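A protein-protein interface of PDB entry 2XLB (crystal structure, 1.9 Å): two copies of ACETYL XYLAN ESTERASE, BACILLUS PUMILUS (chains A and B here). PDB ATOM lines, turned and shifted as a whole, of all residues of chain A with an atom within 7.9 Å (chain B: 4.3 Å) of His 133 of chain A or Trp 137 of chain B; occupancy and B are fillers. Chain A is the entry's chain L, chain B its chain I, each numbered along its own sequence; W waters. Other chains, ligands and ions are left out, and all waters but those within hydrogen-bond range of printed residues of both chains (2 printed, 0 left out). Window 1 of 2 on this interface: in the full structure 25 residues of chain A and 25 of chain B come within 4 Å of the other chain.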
ATOM      1  N   VAL A 128      29.120  25.120   7.548  1.00  0.00           N
ATOM      2  CA  VAL A 128      29.034  24.645   8.928  1.00  0.00           C
ATOM      3  C   VAL A 128      27.683  25.046   9.510  1.00  0.00           C
ATOM      4  O   VAL A 128      27.036  25.965   9.007  1.00  0.00           O
ATOM      5  CB  VAL A 128      30.199  25.253   9.754  1.00  0.00           C
ATOM      6  CG1 VAL A 128      29.976  25.146  11.245  1.00  0.00           C
ATOM      7  CG2 VAL A 128      31.536  24.603   9.343  1.00  0.00           C
ATOM      8  N   THR A 129      27.238  24.345  10.551  1.00  0.00           N
ATOM      9  CA  THR A 129      26.081  24.782  11.330  1.00  0.00           C
ATOM     10  C   THR A 129      26.614  25.602  12.501  1.00  0.00           C
ATOM     11  O   THR A 129      27.222  25.056  13.412  1.00  0.00           O
ATOM     12  CB  THR A 129      25.281  23.593  11.852  1.00  0.00           C
ATOM     13  OG1 THR A 129      24.929  22.747  10.751  1.00  0.00           O
ATOM     14  CG2 THR A 129      24.027  24.068  12.596  1.00  0.00           C
ATOM     15  N   PRO A 130      26.410  26.927  12.471  1.00  0.00           N
ATOM     16  CA  PRO A 130      27.045  27.770  13.481  1.00  0.00           C
ATOM     17  C   PRO A 130      26.497  27.599  14.888  1.00  0.00           C
ATOM     18  O   PRO A 130      27.198  27.849  15.861  1.00  0.00           O
ATOM     19  CB  PRO A 130      26.764  29.198  12.979  1.00  0.00           C
ATOM     20  CG  PRO A 130      26.412  29.059  11.577  1.00  0.00           C
ATOM     21  CD  PRO A 130      25.741  27.731  11.440  1.00  0.00           C
ATOM     22  N   GLY A 131      25.257  27.161  15.005  1.00  0.00           N
ATOM     23  CA  GLY A 131      24.632  27.038  16.313  1.00  0.00           C
ATOM     24  C   GLY A 131      23.297  26.361  16.193  1.00  0.00           C
ATOM     25  O   GLY A 131      23.048  25.674  15.204  1.00  0.00           O
ATOM     26  N   GLY A 132      22.444  26.566  17.192  1.00  0.00           N
ATOM     27  CA  GLY A 132      21.148  25.894  17.252  1.00  0.00           C
ATOM     28  C   GLY A 132      20.212  26.341  16.152  1.00  0.00           C
ATOM     29  O   GLY A 132      20.274  27.477  15.698  1.00  0.00           O
ATOM     30  N   HIS A 133      19.359  25.435  15.699  1.00  0.00           N
ATOM     31  CA  HIS A 133      18.272  25.799  14.800  1.00  0.00           C
ATOM     32  C   HIS A 133      17.104  24.867  14.998  1.00  0.00           C
ATOM     33  O   HIS A 133      17.230  23.829  15.670  1.00  0.00           O
ATOM     34  CB  HIS A 133      18.722  25.871  13.318  1.00  0.00           C
ATOM     35  CG  HIS A 133      19.252  24.592  12.764  1.00  0.00           C
ATOM     36  ND1 HIS A 133      18.485  23.709  12.038  1.00  0.00           N
ATOM     37  CD2 HIS A 133      20.494  24.066  12.802  1.00  0.00           C
ATOM     38  CE1 HIS A 133      19.233  22.676  11.676  1.00  0.00           C
ATOM     39  NE2 HIS A 133      20.457  22.875  12.120  1.00  0.00           N
ATOM     40  N   ALA A 134      15.947  25.279  14.489  1.00  0.00           N
ATOM     41  CA  ALA A 134      14.758  24.446  14.553  1.00  0.00           C
ATOM     42  C   ALA A 134      14.887  23.290  13.558  1.00  0.00           C
ATOM     43  O   ALA A 134      15.641  23.369  12.573  1.00  0.00           O
ATOM     44  CB  ALA A 134      13.506  25.272  14.271  1.00  0.00           C
ATOM     45  N   LEU A 135      14.129  22.230  13.816  1.00  0.00           N
ATOM     46  CA  LEU A 135      14.097  21.070  12.942  1.00  0.00           C
ATOM     47  C   LEU A 135      13.838  21.537  11.506  1.00  0.00           C
ATOM     48  O   LEU A 135      12.822  22.178  11.233  1.00  0.00           O
ATOM     49  CB  LEU A 135      13.018  20.104  13.398  1.00  0.00           C
ATOM     50  CG  LEU A 135      13.140  18.653  12.950  1.00  0.00           C
ATOM     51  CD1 LEU A 135      12.005  17.829  13.577  1.00  0.00           C
ATOM     52  CD2 LEU A 135      13.063  18.621  11.464  1.00  0.00           C
ATOM     53  N   GLY A 136      14.769  21.219  10.614  1.00  0.00           N
ATOM     54  CA  GLY A 136      14.673  21.592   9.220  1.00  0.00           C
ATOM     55  C   GLY A 136      15.854  22.439   8.788  1.00  0.00           C
ATOM     56  O   GLY A 136      16.855  22.552   9.512  1.00  0.00           O
ATOM     57  N   TRP A 137      15.732  23.012   7.592  1.00  0.00           N
ATOM     58  CA  TRP A 137      16.772  23.831   6.997  1.00  0.00           C
ATOM     59  C   TRP A 137      16.493  25.335   7.044  1.00  0.00           C
ATOM     60  O   TRP A 137      17.408  26.138   6.833  1.00  0.00           O
ATOM     61  CB  TRP A 137      16.970  23.438   5.531  1.00  0.00           C
ATOM     62  CG  TRP A 137      17.499  22.062   5.297  1.00  0.00           C
ATOM     63  CD1 TRP A 137      18.805  21.678   5.273  1.00  0.00           C
ATOM     64  CD2 TRP A 137      16.732  20.887   5.012  1.00  0.00           C
ATOM     65  NE1 TRP A 137      18.902  20.326   4.995  1.00  0.00           N
ATOM     66  CE2 TRP A 137      17.639  19.822   4.835  1.00  0.00           C
ATOM     67  CE3 TRP A 137      15.368  20.632   4.900  1.00  0.00           C
ATOM     68  CZ2 TRP A 137      17.222  18.525   4.553  1.00  0.00           C
ATOM     69  CZ3 TRP A 137      14.952  19.345   4.619  1.00  0.00           C
ATOM     70  CH2 TRP A 137      15.878  18.301   4.447  1.00  0.00           C
ATOM     71  N   MET A 138      15.254  25.719   7.321  1.00  0.00           N
ATOM     72  CA  MET A 138      14.841  27.121   7.258  1.00  0.00           C
ATOM     73  C   MET A 138      15.585  28.059   8.197  1.00  0.00           C
ATOM     74  O   MET A 138      15.685  29.239   7.908  1.00  0.00           O
ATOM     75  CB  MET A 138      13.351  27.276   7.588  1.00  0.00           C
ATOM     76  CG  MET A 138      12.406  26.690   6.579  1.00  0.00           C
ATOM     77  SD  MET A 138      12.630  27.430   4.958  1.00  0.00           S
ATOM     78  CE  MET A 138      12.457  29.195   5.294  1.00  0.00           C
ATOM     79  N   THR A 139      16.056  27.552   9.326  1.00  0.00           N
ATOM     80  CA  THR A 139      16.729  28.387  10.300  1.00  0.00           C
ATOM     81  C   THR A 139      18.204  28.009  10.497  1.00  0.00           C
ATOM     82  O   THR A 139      18.857  28.506  11.417  1.00  0.00           O
ATOM     83  CB  THR A 139      15.963  28.389  11.649  1.00  0.00           C
ATOM     84  OG1 THR A 139      15.825  27.060  12.146  1.00  0.00           O
ATOM     85  CG2 THR A 139      14.558  28.951  11.452  1.00  0.00           C
ATOM     86  N   LYS A 140      18.732  27.159   9.628  1.00  0.00           N
ATOM     87  CA  LYS A 140      20.154  26.812   9.682  1.00  0.00           C
ATOM     88  C   LYS A 140      20.999  28.031   9.323  1.00  0.00           C
ATOM     89  O   LYS A 140      20.881  28.568   8.210  1.00  0.00           O
ATOM     90  CB  LYS A 140      20.460  25.636   8.742  1.00  0.00           C
ATOM     91  CG  LYS A 140      21.935  25.227   8.672  1.00  0.00           C
ATOM     92  CD  LYS A 140      22.111  23.938   7.842  1.00  0.00           C
ATOM     93  CE  LYS A 140      23.545  23.428   7.840  1.00  0.00           C
ATOM     94  NZ  LYS A 140      24.403  24.124   6.846  1.00  0.00           N
ATOM     95  N   GLY A 141      21.834  28.469  10.272  1.00  0.00           N
ATOM     96  CA  GLY A 141      22.704  29.635  10.090  1.00  0.00           C
ATOM     97  C   GLY A 141      21.970  30.963  10.025  1.00  0.00           C
ATOM     98  O   GLY A 141      22.467  31.934   9.465  1.00  0.00           O
ATOM     99  N   ILE A 142      20.777  31.004  10.593  1.00  0.00           N
ATOM    100  CA  ILE A 142      19.896  32.180  10.461  1.00  0.00           C
ATOM    101  C   ILE A 142      20.399  33.458  11.171  1.00  0.00           C
ATOM    102  O   ILE A 142      19.879  34.551  10.906  1.00  0.00           O
ATOM    103  CB  ILE A 142      18.464  31.854  10.904  1.00  0.00           C
ATOM    104  CG1 ILE A 142      17.477  32.921  10.386  1.00  0.00           C
ATOM    105  CG2 ILE A 142      18.373  31.704  12.415  1.00  0.00           C
ATOM    106  CD1 ILE A 142      16.039  32.486  10.393  1.00  0.00           C
ATOM    107  N   GLU A 224       8.799  26.727  10.834  1.00  0.00           N
ATOM    108  CA  GLU A 224      10.106  26.433  11.427  1.00  0.00           C
ATOM    109  C   GLU A 224      10.702  27.682  12.084  1.00  0.00           C
ATOM    110  O   GLU A 224      11.434  27.584  13.089  1.00  0.00           O
ATOM    111  CB  GLU A 224      11.084  25.893  10.398  1.00  0.00           C
ATOM    112  CG  GLU A 224      10.737  24.506   9.869  1.00  0.00           C
ATOM    113  CD  GLU A 224      11.763  23.971   8.871  1.00  0.00           C
ATOM    114  OE1 GLU A 224      12.937  24.447   8.866  1.00  0.00           O
ATOM    115  OE2 GLU A 224      11.402  23.022   8.114  1.00  0.00           O
ATOM    116  N   SER A 227       9.041  28.071  15.330  1.00  0.00           N
ATOM    117  CA  SER A 227       9.663  27.050  16.175  1.00  0.00           C
ATOM    118  C   SER A 227      10.999  27.524  16.736  1.00  0.00           C
ATOM    119  O   SER A 227      11.303  27.324  17.911  1.00  0.00           O
ATOM    120  CB  SER A 227       9.872  25.760  15.369  1.00  0.00           C
ATOM    121  OG  SER A 227       8.681  25.013  15.341  1.00  0.00           O
ATOM    122  N   TYR A 228      11.779  28.161  15.873  1.00  0.00           N
ATOM    123  CA  TYR A 228      13.094  28.668  16.245  1.00  0.00           C
ATOM    124  C   TYR A 228      12.980  29.737  17.345  1.00  0.00           C
ATOM    125  O   TYR A 228      13.729  29.728  18.313  1.00  0.00           O
ATOM    126  CB  TYR A 228      13.799  29.223  15.003  1.00  0.00           C
ATOM    127  CG  TYR A 228      15.147  29.842  15.289  1.00  0.00           C
ATOM    128  CD1 TYR A 228      15.298  31.215  15.379  1.00  0.00           C
ATOM    129  CD2 TYR A 228      16.257  29.050  15.515  1.00  0.00           C
ATOM    130  CE1 TYR A 228      16.531  31.786  15.651  1.00  0.00           C
ATOM    131  CE2 TYR A 228      17.495  29.611  15.796  1.00  0.00           C
ATOM    132  CZ  TYR A 228      17.624  30.984  15.857  1.00  0.00           C
ATOM    133  OH  TYR A 228      18.854  31.551  16.134  1.00  0.00           O
ATOM    134  N   ARG A 231      12.279  28.380  20.802  1.00  0.00           N
ATOM    135  CA  ARG A 231      13.458  27.767  21.410  1.00  0.00           C
ATOM    136  C   ARG A 231      14.533  28.784  21.803  1.00  0.00           C
ATOM    137  O   ARG A 231      15.329  28.540  22.701  1.00  0.00           O
ATOM    138  CB  ARG A 231      14.029  26.708  20.470  1.00  0.00           C
ATOM    139  CG  ARG A 231      13.175  25.473  20.410  1.00  0.00           C
ATOM    140  CD  ARG A 231      13.371  24.691  19.124  1.00  0.00           C
ATOM    141  NE  ARG A 231      12.608  23.449  19.171  1.00  0.00           N
ATOM    142  CZ  ARG A 231      11.287  23.363  19.054  1.00  0.00           C
ATOM    143  NH1 ARG A 231      10.553  24.452  18.864  1.00  0.00           N
ATOM    144  NH2 ARG A 231      10.694  22.181  19.131  1.00  0.00           N
ATOM    145  N   ASN A 232      14.523  29.935  21.147  1.00  0.00           N
ATOM    146  CA  ASN A 232      15.525  30.969  21.365  1.00  0.00           C
ATOM    147  C   ASN A 232      14.809  32.307  21.538  1.00  0.00           C
ATOM    148  O   ASN A 232      14.526  33.012  20.579  1.00  0.00           O
ATOM    149  CB  ASN A 232      16.481  30.977  20.178  1.00  0.00           C
ATOM    150  CG  ASN A 232      17.086  29.595  19.914  1.00  0.00           C
ATOM    151  OD1 ASN A 232      18.055  29.201  20.557  1.00  0.00           O
ATOM    152  ND2 ASN A 232      16.484  28.846  18.996  1.00  0.00           N
ATOM    153  N   TYR B  91      15.555  15.488  21.733  1.00  0.00           N
ATOM    154  CA  TYR B  91      15.683  15.788  20.305  1.00  0.00           C
ATOM    155  C   TYR B  91      14.840  17.012  19.962  1.00  0.00           C
ATOM    156  O   TYR B  91      13.628  17.011  20.175  1.00  0.00           O
ATOM    157  CB  TYR B  91      15.202  14.585  19.500  1.00  0.00           C
ATOM    158  CG  TYR B  91      15.440  14.668  18.019  1.00  0.00           C
ATOM    159  CD1 TYR B  91      16.647  14.262  17.468  1.00  0.00           C
ATOM    160  CD2 TYR B  91      14.434  15.073  17.162  1.00  0.00           C
ATOM    161  CE1 TYR B  91      16.855  14.293  16.121  1.00  0.00           C
ATOM    162  CE2 TYR B  91      14.642  15.130  15.804  1.00  0.00           C
ATOM    163  CZ  TYR B  91      15.850  14.734  15.288  1.00  0.00           C
ATOM    164  OH  TYR B  91      16.075  14.755  13.948  1.00  0.00           O
ATOM    165  N   ASN B  92      15.484  18.062  19.448  1.00  0.00           N
ATOM    166  CA  ASN B  92      14.793  19.287  19.069  1.00  0.00           C
ATOM    167  C   ASN B  92      13.964  19.869  20.218  1.00  0.00           C
ATOM    168  O   ASN B  92      12.962  20.535  19.988  1.00  0.00           O
ATOM    169  CB  ASN B  92      13.892  19.011  17.866  1.00  0.00           C
ATOM    170  CG  ASN B  92      13.349  20.277  17.229  1.00  0.00           C
ATOM    171  OD1 ASN B  92      14.075  21.253  17.028  1.00  0.00           O
ATOM    172  ND2 ASN B  92      12.070  20.257  16.895  1.00  0.00           N
ATOM    173  N   GLY B 119      23.933  21.868  16.658  1.00  0.00           N
ATOM    174  CA  GLY B 119      22.907  22.221  15.693  1.00  0.00           C
ATOM    175  C   GLY B 119      21.499  22.292  16.251  1.00  0.00           C
ATOM    176  O   GLY B 119      20.627  22.932  15.674  1.00  0.00           O
ATOM    177  N   GLN B 120      21.261  21.633  17.374  1.00  0.00           N
ATOM    178  CA  GLN B 120      19.931  21.656  17.944  1.00  0.00           C
ATOM    179  C   GLN B 120      19.768  22.827  18.885  1.00  0.00           C
ATOM    180  O   GLN B 120      19.243  23.859  18.504  1.00  0.00           O
ATOM    181  CB  GLN B 120      19.602  20.356  18.673  1.00  0.00           C
ATOM    182  CG  GLN B 120      19.300  19.201  17.763  1.00  0.00           C
ATOM    183  CD  GLN B 120      19.177  17.893  18.515  1.00  0.00           C
ATOM    184  OE1 GLN B 120      18.441  17.788  19.484  1.00  0.00           O
ATOM    185  NE2 GLN B 120      19.897  16.890  18.057  1.00  0.00           N
ATOM    186  N   GLY B 136      15.435  16.891   9.277  1.00  0.00           N
ATOM    187  CA  GLY B 136      15.894  16.579  10.630  1.00  0.00           C
ATOM    188  C   GLY B 136      17.364  16.217  10.659  1.00  0.00           C
ATOM    189  O   GLY B 136      18.079  16.414   9.684  1.00  0.00           O
ATOM    190  N   TRP B 137      17.812  15.700  11.799  1.00  0.00           N
ATOM    191  CA  TRP B 137      19.213  15.357  12.015  1.00  0.00           C
ATOM    192  C   TRP B 137      19.490  13.859  11.956  1.00  0.00           C
ATOM    193  O   TRP B 137      20.658  13.452  11.866  1.00  0.00           O
ATOM    194  CB  TRP B 137      19.685  15.871  13.374  1.00  0.00           C
ATOM    195  CG  TRP B 137      19.727  17.386  13.502  1.00  0.00           C
ATOM    196  CD1 TRP B 137      20.759  18.213  13.150  1.00  0.00           C
ATOM    197  CD2 TRP B 137      18.710  18.221  14.043  1.00  0.00           C
ATOM    198  NE1 TRP B 137      20.434  19.522  13.430  1.00  0.00           N
ATOM    199  CE2 TRP B 137      19.179  19.553  13.978  1.00  0.00           C
ATOM    200  CE3 TRP B 137      17.438  17.978  14.574  1.00  0.00           C
ATOM    201  CZ2 TRP B 137      18.426  20.627  14.424  1.00  0.00           C
ATOM    202  CZ3 TRP B 137      16.685  19.052  15.017  1.00  0.00           C
ATOM    203  CH2 TRP B 137      17.183  20.365  14.941  1.00  0.00           C
ATOM    204  N   MET B 138      18.439  13.046  12.022  1.00  0.00           N
ATOM    205  CA  MET B 138      18.592  11.587  12.149  1.00  0.00           C
ATOM    206  C   MET B 138      19.297  10.926  10.982  1.00  0.00           C
ATOM    207  O   MET B 138      19.877   9.866  11.162  1.00  0.00           O
ATOM    208  CB  MET B 138      17.232  10.901  12.289  1.00  0.00           C
ATOM    209  CG  MET B 138      16.505  11.185  13.567  1.00  0.00           C
ATOM    210  SD  MET B 138      17.474  10.637  14.996  1.00  0.00           S
ATOM    211  CE  MET B 138      17.730   8.916  14.601  1.00  0.00           C
ATOM    212  N   THR B 139      19.205  11.512   9.789  1.00  0.00           N
ATOM    213  CA  THR B 139      19.815  10.906   8.606  1.00  0.00           C
ATOM    214  C   THR B 139      20.947  11.748   8.011  1.00  0.00           C
ATOM    215  O   THR B 139      21.469  11.433   6.947  1.00  0.00           O
ATOM    216  CB  THR B 139      18.746  10.533   7.557  1.00  0.00           C
ATOM    217  OG1 THR B 139      18.003  11.697   7.181  1.00  0.00           O
ATOM    218  CG2 THR B 139      17.773   9.496   8.145  1.00  0.00           C
ATOM    219  N   LYS B 140      21.358  12.794   8.721  1.00  0.00           N
ATOM    220  CA  LYS B 140      22.477  13.619   8.270  1.00  0.00           C
ATOM    221  C   LYS B 140      23.777  12.800   8.305  1.00  0.00           C
ATOM    222  O   LYS B 140      24.219  12.325   9.369  1.00  0.00           O
ATOM    223  CB  LYS B 140      22.591  14.877   9.137  1.00  0.00           C
ATOM    224  CG  LYS B 140      23.768  15.800   8.785  1.00  0.00           C
ATOM    225  CD  LYS B 140      23.701  17.110   9.586  1.00  0.00           C
ATOM    226  CE  LYS B 140      24.795  18.094   9.183  1.00  0.00           C
ATOM    227  NZ  LYS B 140      26.109  17.753   9.788  1.00  0.00           N
ATOM    228  N   TYR B 149      25.790  12.112  11.899  1.00  0.00           N
ATOM    229  CA  TYR B 149      25.511  13.184  12.852  1.00  0.00           C
ATOM    230  C   TYR B 149      25.906  12.832  14.287  1.00  0.00           C
ATOM    231  O   TYR B 149      26.523  13.629  14.977  1.00  0.00           O
ATOM    232  CB  TYR B 149      24.013  13.509  12.816  1.00  0.00           C
ATOM    233  CG  TYR B 149      23.582  14.556  13.816  1.00  0.00           C
ATOM    234  CD1 TYR B 149      22.739  14.229  14.871  1.00  0.00           C
ATOM    235  CD2 TYR B 149      24.052  15.868  13.729  1.00  0.00           C
ATOM    236  CE1 TYR B 149      22.340  15.177  15.780  1.00  0.00           C
ATOM    237  CE2 TYR B 149      23.661  16.835  14.650  1.00  0.00           C
ATOM    238  CZ  TYR B 149      22.809  16.477  15.675  1.00  0.00           C
ATOM    239  OH  TYR B 149      22.401  17.426  16.582  1.00  0.00           O
ATOM    240  N   GLU B 224      12.048   9.579  10.576  1.00  0.00           N
ATOM    241  CA  GLU B 224      12.932  10.287   9.647  1.00  0.00           C
ATOM    242  C   GLU B 224      13.725   9.299   8.791  1.00  0.00           C
ATOM    243  O   GLU B 224      14.016   9.564   7.628  1.00  0.00           O
ATOM    244  CB  GLU B 224      13.897  11.202  10.385  1.00  0.00           C
ATOM    245  CG  GLU B 224      13.264  12.420  11.012  1.00  0.00           C
ATOM    246  CD  GLU B 224      14.283  13.329  11.697  1.00  0.00           C
ATOM    247  OE1 GLU B 224      15.477  13.270  11.332  1.00  0.00           O
ATOM    248  OE2 GLU B 224      13.888  14.124  12.578  1.00  0.00           O
HETATM  249  O   HOH W   1      15.666  22.605  20.576  1.00  0.00           O
HETATM  250  O   HOH W   2      10.577  22.157  15.573  1.00  0.00           O
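Of chain A, only His 133 (3.5 Å), Ala 134 (3.97 Å) and Leu 135 (3.7 Å) come within 4 Å of Trp 137 of chain B.
Printed residues of chain A within 4 Å of Gly 136 of chain B: Leu 135 (3.6 Å).
Printed residues of chain A within 4 Å of Gln 120 of chain B: Gly 132 (3.1 Å) and His 133 (3.2 Å).
Of the printed residues of chain B, Leu 135 of chain A touches Asn 92, Gly 136 and Trp 137.
Printed residues of chain A within 4 Å of Gly 119 of chain B: Thr 129 (3.8 Å), Gly 131 (3.5 Å), Gly 132 (3.4 Å) and His 133 (2.8 Å).
Printed residues of chain B within 4 Å of Thr 129 of chain A: Gly 119 (3.8 Å).
The nearest residue of chain A that does not touch Trp 137 of chain B is Gly 136 of chain A (5.0 Å).
6 positions are printed for both chains.
OD1 of Asn 92 of chain B sits at hydrogen-bond distance from N of Leu 135 of chain A.
The backbone NH of His 133 of chain A sits at hydrogen-bond distance from the backbone carbonyl oxygen of Gly 119 of chain B, at 2.8 Å.
The backbone carbonyl oxygen of Asn 92 of chain B sits at hydrogen-bond distance from the guanidinium group of Arg 231 of chain A (2.9 Å).
The backbone carbonyl oxygen of Gln 120 of chain B lies within hydrogen-bond range of the backbone NH of His 133 of chain A, 3.2 Å away.
Thr 129 of chain A touches Gly 119 of chain B.
Gly 131 of chain A touches Gly 119 of chain B.
O of Gly 119 of chain B touches CA of Gly 132 of chain A, 3.4 Å away.
Gly 132 of chain A touches Gln 120 of chain B.
CE1 of His 133 of chain A touches CZ2 of Trp 137 of chain B, at 3.5 Å.
C of Ala 134 of chain A touches CH2 of Trp 137 of chain B (3.97 Å).
Gly 136 of chain B touches Leu 135 of chain A.
Leu 135 of chain A touches Trp 137 of chain B (CA to CH2, 3.7 Å).
Of the 20 printed residues of chain A, 7 touch a printed residue of chain B.
Hydrophobic or aromatic side chains of chain A within 4 Å of the printed part of chain B: His 133 and Leu 135.
Hydrophobic or aromatic side chains of chain B that line the printed part of chain A: Trp 137.
Along chain B the printed residues that touch a printed residue of chain A span positions 92 to 137.
Among the printed residues, no Asp or Glu carboxylate lies within 4 Å of a Lys or Arg side-chain nitrogen of the other chain.
The side-chain amide oxygen of Gln 120 of chain B sits at hydrogen-bond distance from the backbone NH of Asn 92 of chain B, 3.0 Å away.
The side-chain amide nitrogen (NE2) of Gln 120 of chain B sits at hydrogen-bond distance from the side-chain hydroxyl (OH) of Tyr 149 of chain B (3.0 Å).
ND1 of His 133 of chain A sits close to O of Gly 136 of chain A.
N of Trp 137 of chain B sits at hydrogen-bond distance from OE1 of Glu 224 of chain B (3.4 Å).
The backbone carbonyl oxygen (O) of Ser 227 of chain A sits at hydrogen-bond distance from the guanidinium group (NH1) of Arg 231 of chain A, at 3.1 Å.
The backbone NH (N) of Ala 134 of chain A is in hydrogen-bond range of the side-chain hydroxyl (OG1) of Thr 139 of chain A.
Water W2 bridges ND2 of Asn 92 of chain B (2.8 Å) and OG of Ser 227 of chain A (3.4 Å).
Water W1 bridges O of Asn 92 of chain B (3.5 Å) and NE of Arg 231 of chain A (3.5 Å).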
